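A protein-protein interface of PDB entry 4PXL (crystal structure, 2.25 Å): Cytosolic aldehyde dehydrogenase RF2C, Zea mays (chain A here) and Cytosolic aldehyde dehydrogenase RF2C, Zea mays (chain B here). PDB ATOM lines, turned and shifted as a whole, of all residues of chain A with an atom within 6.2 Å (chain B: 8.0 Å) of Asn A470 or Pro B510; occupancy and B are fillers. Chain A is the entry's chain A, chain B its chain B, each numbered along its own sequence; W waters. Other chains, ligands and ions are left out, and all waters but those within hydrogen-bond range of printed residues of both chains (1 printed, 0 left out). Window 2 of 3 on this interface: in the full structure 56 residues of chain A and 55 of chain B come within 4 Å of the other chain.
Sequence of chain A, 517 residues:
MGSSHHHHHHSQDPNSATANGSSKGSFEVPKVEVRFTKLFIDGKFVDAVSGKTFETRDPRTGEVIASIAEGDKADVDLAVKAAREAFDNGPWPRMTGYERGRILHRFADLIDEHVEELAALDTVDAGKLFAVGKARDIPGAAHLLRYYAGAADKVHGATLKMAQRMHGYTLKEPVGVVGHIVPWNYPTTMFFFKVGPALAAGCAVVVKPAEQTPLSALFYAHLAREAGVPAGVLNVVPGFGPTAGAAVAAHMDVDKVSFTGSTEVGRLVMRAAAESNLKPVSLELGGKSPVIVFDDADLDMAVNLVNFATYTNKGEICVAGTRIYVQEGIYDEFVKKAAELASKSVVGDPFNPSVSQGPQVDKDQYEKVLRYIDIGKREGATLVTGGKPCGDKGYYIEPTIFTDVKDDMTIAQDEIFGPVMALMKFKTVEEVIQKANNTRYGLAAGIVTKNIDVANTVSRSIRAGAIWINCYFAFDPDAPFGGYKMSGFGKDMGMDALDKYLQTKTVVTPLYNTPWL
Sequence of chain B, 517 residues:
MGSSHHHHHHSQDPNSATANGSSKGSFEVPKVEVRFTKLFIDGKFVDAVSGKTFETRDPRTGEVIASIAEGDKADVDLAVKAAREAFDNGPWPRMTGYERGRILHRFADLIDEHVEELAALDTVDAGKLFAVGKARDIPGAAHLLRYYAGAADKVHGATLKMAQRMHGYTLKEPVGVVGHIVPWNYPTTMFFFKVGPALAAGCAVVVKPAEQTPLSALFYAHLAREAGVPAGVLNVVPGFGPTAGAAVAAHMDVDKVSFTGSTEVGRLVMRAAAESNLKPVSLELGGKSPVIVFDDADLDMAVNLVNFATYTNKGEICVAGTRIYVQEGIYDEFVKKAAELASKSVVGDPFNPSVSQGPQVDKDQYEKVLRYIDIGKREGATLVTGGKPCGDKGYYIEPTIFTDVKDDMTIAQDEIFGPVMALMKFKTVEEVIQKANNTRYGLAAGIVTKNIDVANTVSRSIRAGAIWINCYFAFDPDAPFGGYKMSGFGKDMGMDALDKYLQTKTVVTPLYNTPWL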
ATOM      1  N   ALA A 297     -10.699  31.955 -15.625  1.00  0.00           N
ATOM      2  CA  ALA A 297     -10.563  30.506 -15.495  1.00  0.00           C
ATOM      3  C   ALA A 297     -11.805  29.745 -16.027  1.00  0.00           C
ATOM      4  O   ALA A 297     -12.915  30.288 -16.046  1.00  0.00           O
ATOM      5  CB  ALA A 297     -10.325  30.150 -14.032  1.00  0.00           C
ATOM      6  N   MET A 301     -13.096  23.401 -14.370  1.00  0.00           N
ATOM      7  CA  MET A 301     -11.706  23.017 -14.129  1.00  0.00           C
ATOM      8  C   MET A 301     -11.241  23.586 -12.762  1.00  0.00           C
ATOM      9  O   MET A 301     -10.716  22.832 -11.937  1.00  0.00           O
ATOM     10  CB  MET A 301     -10.826  23.497 -15.303  1.00  0.00           C
ATOM     11  CG  MET A 301      -9.318  23.367 -15.074  1.00  0.00           C
ATOM     12  SD  MET A 301      -8.612  24.791 -14.211  1.00  0.00           S
ATOM     13  CE  MET A 301      -9.121  26.202 -15.428  1.00  0.00           C
ATOM     14  N   LEU A 305     -10.201  21.563  -9.367  1.00  0.00           N
ATOM     15  CA  LEU A 305      -8.829  21.759  -8.922  1.00  0.00           C
ATOM     16  C   LEU A 305      -8.750  22.170  -7.444  1.00  0.00           C
ATOM     17  O   LEU A 305      -7.934  21.627  -6.690  1.00  0.00           O
ATOM     18  CB  LEU A 305      -8.133  22.775  -9.856  1.00  0.00           C
ATOM     19  CG  LEU A 305      -6.609  22.987  -9.712  1.00  0.00           C
ATOM     20  CD1 LEU A 305      -5.836  21.673  -9.904  1.00  0.00           C
ATOM     21  CD2 LEU A 305      -6.117  24.029 -10.729  1.00  0.00           C
ATOM     22  N   GLY A 446      -1.380  28.182  -5.313  1.00  0.00           N
ATOM     23  CA  GLY A 446      -1.981  27.810  -6.579  1.00  0.00           C
ATOM     24  C   GLY A 446      -2.553  29.037  -7.255  1.00  0.00           C
ATOM     25  O   GLY A 446      -3.068  29.926  -6.578  1.00  0.00           O
ATOM     26  N   ILE A 447      -2.419  29.122  -8.581  1.00  0.00           N
ATOM     27  CA  ILE A 447      -2.945  30.223  -9.387  1.00  0.00           C
ATOM     28  C   ILE A 447      -3.732  29.592 -10.515  1.00  0.00           C
ATOM     29  O   ILE A 447      -3.227  28.677 -11.163  1.00  0.00           O
ATOM     30  CB  ILE A 447      -1.837  31.144  -9.953  1.00  0.00           C
ATOM     31  CG1 ILE A 447      -0.935  31.696  -8.862  1.00  0.00           C
ATOM     32  CG2 ILE A 447      -2.424  32.269 -10.808  1.00  0.00           C
ATOM     33  CD1 ILE A 447       0.423  32.200  -9.439  1.00  0.00           C
ATOM     34  N   VAL A 448      -4.970  30.068 -10.742  1.00  0.00           N
ATOM     35  CA  VAL A 448      -5.801  29.588 -11.837  1.00  0.00           C
ATOM     36  C   VAL A 448      -6.139  30.781 -12.727  1.00  0.00           C
ATOM     37  O   VAL A 448      -6.931  31.638 -12.333  1.00  0.00           O
ATOM     38  CB  VAL A 448      -7.067  28.784 -11.408  1.00  0.00           C
ATOM     39  CG1 VAL A 448      -7.686  28.089 -12.620  1.00  0.00           C
ATOM     40  CG2 VAL A 448      -6.738  27.760 -10.328  1.00  0.00           C
ATOM     41  N   THR A 449      -5.481  30.862 -13.897  1.00  0.00           N
ATOM     42  CA  THR A 449      -5.653  31.924 -14.907  1.00  0.00           C
ATOM     43  C   THR A 449      -5.131  31.419 -16.258  1.00  0.00           C
ATOM     44  O   THR A 449      -4.248  30.565 -16.295  1.00  0.00           O
ATOM     45  CB  THR A 449      -4.963  33.260 -14.496  1.00  0.00           C
ATOM     46  OG1 THR A 449      -5.413  34.292 -15.353  1.00  0.00           O
ATOM     47  CG2 THR A 449      -3.450  33.219 -14.585  1.00  0.00           C
ATOM     48  N   LYS A 450      -5.627  31.990 -17.349  1.00  0.00           N
ATOM     49  CA  LYS A 450      -5.173  31.647 -18.689  1.00  0.00           C
ATOM     50  C   LYS A 450      -4.206  32.724 -19.195  1.00  0.00           C
ATOM     51  O   LYS A 450      -3.511  32.509 -20.183  1.00  0.00           O
ATOM     52  CB  LYS A 450      -6.384  31.587 -19.626  1.00  0.00           C
ATOM     53  CG  LYS A 450      -7.415  30.510 -19.279  1.00  0.00           C
ATOM     54  CD  LYS A 450      -8.546  30.505 -20.299  1.00  0.00           C
ATOM     55  CE  LYS A 450      -9.448  29.324 -20.104  1.00  0.00           C
ATOM     56  NZ  LYS A 450     -10.681  29.446 -20.932  1.00  0.00           N
ATOM     57  N   TRP A 468       1.997  26.702  -8.229  1.00  0.00           N
ATOM     58  CA  TRP A 468       1.346  25.774  -9.150  1.00  0.00           C
ATOM     59  C   TRP A 468       0.314  26.513  -9.957  1.00  0.00           C
ATOM     60  O   TRP A 468      -0.672  26.999  -9.417  1.00  0.00           O
ATOM     61  CB  TRP A 468       0.775  24.557  -8.395  1.00  0.00           C
ATOM     62  CG  TRP A 468       1.838  23.765  -7.701  1.00  0.00           C
ATOM     63  CD1 TRP A 468       3.084  23.475  -8.185  1.00  0.00           C
ATOM     64  CD2 TRP A 468       1.775  23.193  -6.387  1.00  0.00           C
ATOM     65  NE1 TRP A 468       3.801  22.770  -7.254  1.00  0.00           N
ATOM     66  CE2 TRP A 468       3.029  22.585  -6.135  1.00  0.00           C
ATOM     67  CE3 TRP A 468       0.806  23.182  -5.369  1.00  0.00           C
ATOM     68  CZ2 TRP A 468       3.306  21.895  -4.937  1.00  0.00           C
ATOM     69  CZ3 TRP A 468       1.094  22.530  -4.173  1.00  0.00           C
ATOM     70  CH2 TRP A 468       2.326  21.891  -3.970  1.00  0.00           C
ATOM     71  N   ILE A 469       0.602  26.678 -11.252  1.00  0.00           N
ATOM     72  CA  ILE A 469      -0.245  27.404 -12.164  1.00  0.00           C
ATOM     73  C   ILE A 469      -1.091  26.445 -12.955  1.00  0.00           C
ATOM     74  O   ILE A 469      -0.548  25.651 -13.709  1.00  0.00           O
ATOM     75  CB  ILE A 469       0.587  28.359 -13.065  1.00  0.00           C
ATOM     76  CG1 ILE A 469       1.502  29.266 -12.193  1.00  0.00           C
ATOM     77  CG2 ILE A 469      -0.362  29.201 -13.967  1.00  0.00           C
ATOM     78  CD1 ILE A 469       2.520  30.127 -12.950  1.00  0.00           C
ATOM     79  N   ASN A 470      -2.427  26.518 -12.795  1.00  0.00           N
ATOM     80  CA  ASN A 470      -3.391  25.671 -13.517  1.00  0.00           C
ATOM     81  C   ASN A 470      -3.222  24.161 -13.254  1.00  0.00           C
ATOM     82  O   ASN A 470      -3.533  23.333 -14.117  1.00  0.00           O
ATOM     83  CB  ASN A 470      -3.370  25.999 -15.021  1.00  0.00           C
ATOM     84  CG  ASN A 470      -3.794  27.415 -15.272  1.00  0.00           C
ATOM     85  OD1 ASN A 470      -4.663  27.941 -14.584  1.00  0.00           O
ATOM     86  ND2 ASN A 470      -3.157  28.073 -16.231  1.00  0.00           N
ATOM     87  N   CYS A 471      -2.718  23.833 -12.049  1.00  0.00           N
ATOM     88  CA  CYS A 471      -2.440  22.481 -11.565  1.00  0.00           C
ATOM     89  C   CYS A 471      -2.257  22.602 -10.075  1.00  0.00           C
ATOM     90  O   CYS A 471      -2.216  23.715  -9.541  1.00  0.00           O
ATOM     91  CB  CYS A 471      -1.200  21.877 -12.242  1.00  0.00           C
ATOM     92  SG  CYS A 471       0.352  22.775 -11.933  1.00  0.00           S
ATOM     93  N   TYR A 472      -2.136  21.479  -9.394  1.00  0.00           N
ATOM     94  CA  TYR A 472      -1.891  21.469  -7.953  1.00  0.00           C
ATOM     95  C   TYR A 472      -1.129  20.233  -7.547  1.00  0.00           C
ATOM     96  O   TYR A 472      -1.232  19.217  -8.238  1.00  0.00           O
ATOM     97  CB  TYR A 472      -3.189  21.638  -7.139  1.00  0.00           C
ATOM     98  CG  TYR A 472      -2.912  22.412  -5.873  1.00  0.00           C
ATOM     99  CD1 TYR A 472      -2.713  23.789  -5.906  1.00  0.00           C
ATOM    100  CD2 TYR A 472      -2.722  21.754  -4.658  1.00  0.00           C
ATOM    101  CE1 TYR A 472      -2.385  24.502  -4.754  1.00  0.00           C
ATOM    102  CE2 TYR A 472      -2.452  22.464  -3.490  1.00  0.00           C
ATOM    103  CZ  TYR A 472      -2.268  23.839  -3.548  1.00  0.00           C
ATOM    104  OH  TYR A 472      -1.996  24.575  -2.427  1.00  0.00           O
ATOM    105  N   GLN B 164       6.086  14.281 -15.717  1.00  0.00           N
ATOM    106  CA  GLN B 164       4.673  14.424 -16.129  1.00  0.00           C
ATOM    107  C   GLN B 164       4.617  15.420 -17.270  1.00  0.00           C
ATOM    108  O   GLN B 164       5.623  16.079 -17.554  1.00  0.00           O
ATOM    109  CB  GLN B 164       3.831  14.947 -14.970  1.00  0.00           C
ATOM    110  CG  GLN B 164       3.399  13.850 -14.002  1.00  0.00           C
ATOM    111  CD  GLN B 164       2.502  14.386 -12.921  1.00  0.00           C
ATOM    112  OE1 GLN B 164       2.977  14.850 -11.877  1.00  0.00           O
ATOM    113  NE2 GLN B 164       1.185  14.362 -13.170  1.00  0.00           N
ATOM    114  N   ARG B 165       3.441  15.582 -17.904  1.00  0.00           N
ATOM    115  CA  ARG B 165       3.285  16.513 -19.020  1.00  0.00           C
ATOM    116  C   ARG B 165       3.149  17.917 -18.419  1.00  0.00           C
ATOM    117  O   ARG B 165       2.069  18.500 -18.362  1.00  0.00           O
ATOM    118  CB  ARG B 165       2.078  16.114 -19.900  1.00  0.00           C
ATOM    119  CG  ARG B 165       2.331  16.272 -21.399  1.00  0.00           C
ATOM    120  CD  ARG B 165       1.267  15.611 -22.278  1.00  0.00           C
ATOM    121  NE  ARG B 165       1.189  14.153 -22.072  1.00  0.00           N
ATOM    122  CZ  ARG B 165       0.415  13.320 -22.766  1.00  0.00           C
ATOM    123  NH1 ARG B 165      -0.346  13.775 -23.756  1.00  0.00           N
ATOM    124  NH2 ARG B 165       0.411  12.022 -22.489  1.00  0.00           N
ATOM    125  N   MET B 166       4.266  18.432 -17.928  1.00  0.00           N
ATOM    126  CA  MET B 166       4.318  19.710 -17.229  1.00  0.00           C
ATOM    127  C   MET B 166       5.603  20.421 -17.512  1.00  0.00           C
ATOM    128  O   MET B 166       6.612  19.771 -17.777  1.00  0.00           O
ATOM    129  CB  MET B 166       4.235  19.474 -15.699  1.00  0.00           C
ATOM    130  CG  MET B 166       2.916  18.893 -15.236  1.00  0.00           C
ATOM    131  SD  MET B 166       2.734  18.820 -13.445  1.00  0.00           S
ATOM    132  CE  MET B 166       4.005  17.690 -13.014  1.00  0.00           C
ATOM    133  N   HIS B 167       5.593  21.747 -17.375  1.00  0.00           N
ATOM    134  CA  HIS B 167       6.773  22.595 -17.520  1.00  0.00           C
ATOM    135  C   HIS B 167       7.104  23.148 -16.146  1.00  0.00           C
ATOM    136  O   HIS B 167       6.284  23.808 -15.537  1.00  0.00           O
ATOM    137  CB  HIS B 167       6.533  23.734 -18.516  1.00  0.00           C
ATOM    138  CG  HIS B 167       7.642  24.742 -18.572  1.00  0.00           C
ATOM    139  ND1 HIS B 167       8.990  24.357 -18.607  1.00  0.00           N
ATOM    140  CD2 HIS B 167       7.574  26.092 -18.585  1.00  0.00           C
ATOM    141  CE1 HIS B 167       9.681  25.483 -18.605  1.00  0.00           C
ATOM    142  NE2 HIS B 167       8.873  26.555 -18.603  1.00  0.00           N
ATOM    143  N   GLY B 168       8.286  22.815 -15.645  1.00  0.00           N
ATOM    144  CA  GLY B 168       8.743  23.276 -14.342  1.00  0.00           C
ATOM    145  C   GLY B 168      10.002  24.105 -14.459  1.00  0.00           C
ATOM    146  O   GLY B 168      10.838  23.864 -15.330  1.00  0.00           O
ATOM    147  N   VAL B 508       5.388  25.603 -11.639  1.00  0.00           N
ATOM    148  CA  VAL B 508       4.972  24.471 -12.489  1.00  0.00           C
ATOM    149  C   VAL B 508       3.627  24.726 -13.133  1.00  0.00           C
ATOM    150  O   VAL B 508       2.714  25.208 -12.479  1.00  0.00           O
ATOM    151  CB  VAL B 508       4.972  23.109 -11.745  1.00  0.00           C
ATOM    152  CG1 VAL B 508       4.669  21.952 -12.700  1.00  0.00           C
ATOM    153  CG2 VAL B 508       6.285  22.868 -10.983  1.00  0.00           C
ATOM    154  N   THR B 509       3.501  24.382 -14.419  1.00  0.00           N
ATOM    155  CA  THR B 509       2.279  24.533 -15.207  1.00  0.00           C
ATOM    156  C   THR B 509       2.119  23.312 -16.106  1.00  0.00           C
ATOM    157  O   THR B 509       3.132  22.759 -16.528  1.00  0.00           O
ATOM    158  CB  THR B 509       2.226  25.903 -15.950  1.00  0.00           C
ATOM    159  OG1 THR B 509       0.876  26.199 -16.328  1.00  0.00           O
ATOM    160  CG2 THR B 509       3.101  25.970 -17.171  1.00  0.00           C
ATOM    161  N   PRO B 510       0.898  22.826 -16.397  1.00  0.00           N
ATOM    162  CA  PRO B 510       0.805  21.675 -17.308  1.00  0.00           C
ATOM    163  C   PRO B 510       1.166  22.073 -18.730  1.00  0.00           C
ATOM    164  O   PRO B 510       1.167  23.259 -19.033  1.00  0.00           O
ATOM    165  CB  PRO B 510      -0.678  21.254 -17.231  1.00  0.00           C
ATOM    166  CG  PRO B 510      -1.358  22.245 -16.375  1.00  0.00           C
ATOM    167  CD  PRO B 510      -0.433  23.331 -15.999  1.00  0.00           C
ATOM    168  N   LEU B 511       1.489  21.087 -19.583  1.00  0.00           N
ATOM    169  CA  LEU B 511       1.746  21.298 -21.030  1.00  0.00           C
ATOM    170  C   LEU B 511       0.695  20.579 -21.873  1.00  0.00           C
ATOM    171  O   LEU B 511       0.245  19.504 -21.494  1.00  0.00           O
ATOM    172  CB  LEU B 511       3.127  20.790 -21.463  1.00  0.00           C
ATOM    173  CG  LEU B 511       4.312  21.551 -20.935  1.00  0.00           C
ATOM    174  CD1 LEU B 511       5.558  20.731 -21.065  1.00  0.00           C
ATOM    175  CD2 LEU B 511       4.375  22.993 -21.492  1.00  0.00           C
ATOM    176  N   TYR B 512       0.358  21.140 -23.033  1.00  0.00           N
ATOM    177  CA  TYR B 512      -0.615  20.596 -23.953  1.00  0.00           C
ATOM    178  C   TYR B 512       0.014  20.466 -25.332  1.00  0.00           C
ATOM    179  O   TYR B 512       0.623  21.424 -25.843  1.00  0.00           O
ATOM    180  CB  TYR B 512      -1.879  21.494 -24.011  1.00  0.00           C
ATOM    181  CG  TYR B 512      -2.510  21.700 -22.649  1.00  0.00           C
ATOM    182  CD1 TYR B 512      -3.365  20.744 -22.102  1.00  0.00           C
ATOM    183  CD2 TYR B 512      -2.202  22.816 -21.875  1.00  0.00           C
ATOM    184  CE1 TYR B 512      -3.869  20.880 -20.809  1.00  0.00           C
ATOM    185  CE2 TYR B 512      -2.729  22.975 -20.595  1.00  0.00           C
ATOM    186  CZ  TYR B 512      -3.573  22.012 -20.073  1.00  0.00           C
ATOM    187  OH  TYR B 512      -4.133  22.193 -18.829  1.00  0.00           O
ATOM    188  N   ASN B 513      -0.174  19.284 -25.956  1.00  0.00           N
ATOM    189  CA  ASN B 513       0.333  19.000 -27.314  1.00  0.00           C
ATOM    190  C   ASN B 513       1.812  19.321 -27.483  1.00  0.00           C
ATOM    191  O   ASN B 513       2.196  19.992 -28.448  1.00  0.00           O
ATOM    192  CB  ASN B 513      -0.498  19.737 -28.393  1.00  0.00           C
ATOM    193  CG  ASN B 513      -1.940  19.323 -28.409  1.00  0.00           C
ATOM    194  OD1 ASN B 513      -2.270  18.134 -28.515  1.00  0.00           O
ATOM    195  ND2 ASN B 513      -2.824  20.303 -28.285  1.00  0.00           N
ATOM    196  N   THR B 514       2.639  18.893 -26.532  1.00  0.00           N
ATOM    197  CA  THR B 514       4.066  19.168 -26.685  1.00  0.00           C
ATOM    198  C   THR B 514       4.716  18.122 -27.625  1.00  0.00           C
ATOM    199  O   THR B 514       4.428  16.930 -27.480  1.00  0.00           O
ATOM    200  CB  THR B 514       4.743  19.379 -25.331  1.00  0.00           C
ATOM    201  OG1 THR B 514       6.078  19.823 -25.575  1.00  0.00           O
ATOM    202  CG2 THR B 514       4.733  18.121 -24.439  1.00  0.00           C
HETATM  203  O   HOH W   1      -1.693  26.209 -17.868  1.00  0.00           O
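Printed residues of chain A within 4 Å of Thr B509: Ile A469.
Printed residues of chain B within 4 Å of Trp A468: Val B508.
Of the printed residues of chain B, Ile A469 touches Val B508 (2.9 Å), Thr B509 (3.0 Å) and Pro B510 (3.3 Å).
Printed residues of chain B within 4 Å of Cys A471: Val B508 (3.4 Å).
Of the printed residues of chain A, Val B508 touches Trp A468, Ile A469 and Cys A471.
The nearest printed residue of chain A that does not touch Val B508 is Asn A470 (5.3 Å).
N of Ile A447 sits at hydrogen-bond distance from O of Trp A468 (2.9 Å).
The backbone carbonyl oxygen (O) of Ile A447 lies within hydrogen-bond range of the backbone NH (N) of Asn A470, 2.8 Å away.
O of Thr A449 is in hydrogen-bond range of ND2 of Asn A470 (2.7 Å).
The backbone carbonyl oxygen (O) of Ile A469 sits at hydrogen-bond distance from the side-chain sulfur (SG) of Cys A471 (3.5 Å).
The backbone carbonyl oxygen (O) of Thr B509 lies within hydrogen-bond range of the backbone NH (N) of His B167 (2.8 Å).
Printed residues of chain B that touch a printed residue of chain A: Val B508, Thr B509 and Pro B510.
Hydrophobic or aromatic side chains of chain B that line the printed part of chain A: Pro B510.
Among the printed residues, no Asp or Glu carboxylate lies within 4 Å of a Lys or Arg side-chain nitrogen of the other chain.
Water W1 bridges ND2 of Asn A470 and OG1 of Thr B509.
Val B508 touches Trp A468 (O to CA, 3.6 Å).
CD of Pro B510 touches O of Ile A469, at 3.3 Å.
O of Asn A470 touches CG of Pro B510 (3.3 Å).
The backbone NH (N) of Ile A469 sits at hydrogen-bond distance from the backbone carbonyl oxygen (O) of Val B508, at 2.9 Å.
The backbone carbonyl oxygen (O) of Ile A469 is in hydrogen-bond range of the side-chain hydroxyl (OG1) of Thr B509, at 3.0 Å.
SG of Cys A471 lies within hydrogen-bond range of O of Val B508, 3.4 Å away.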
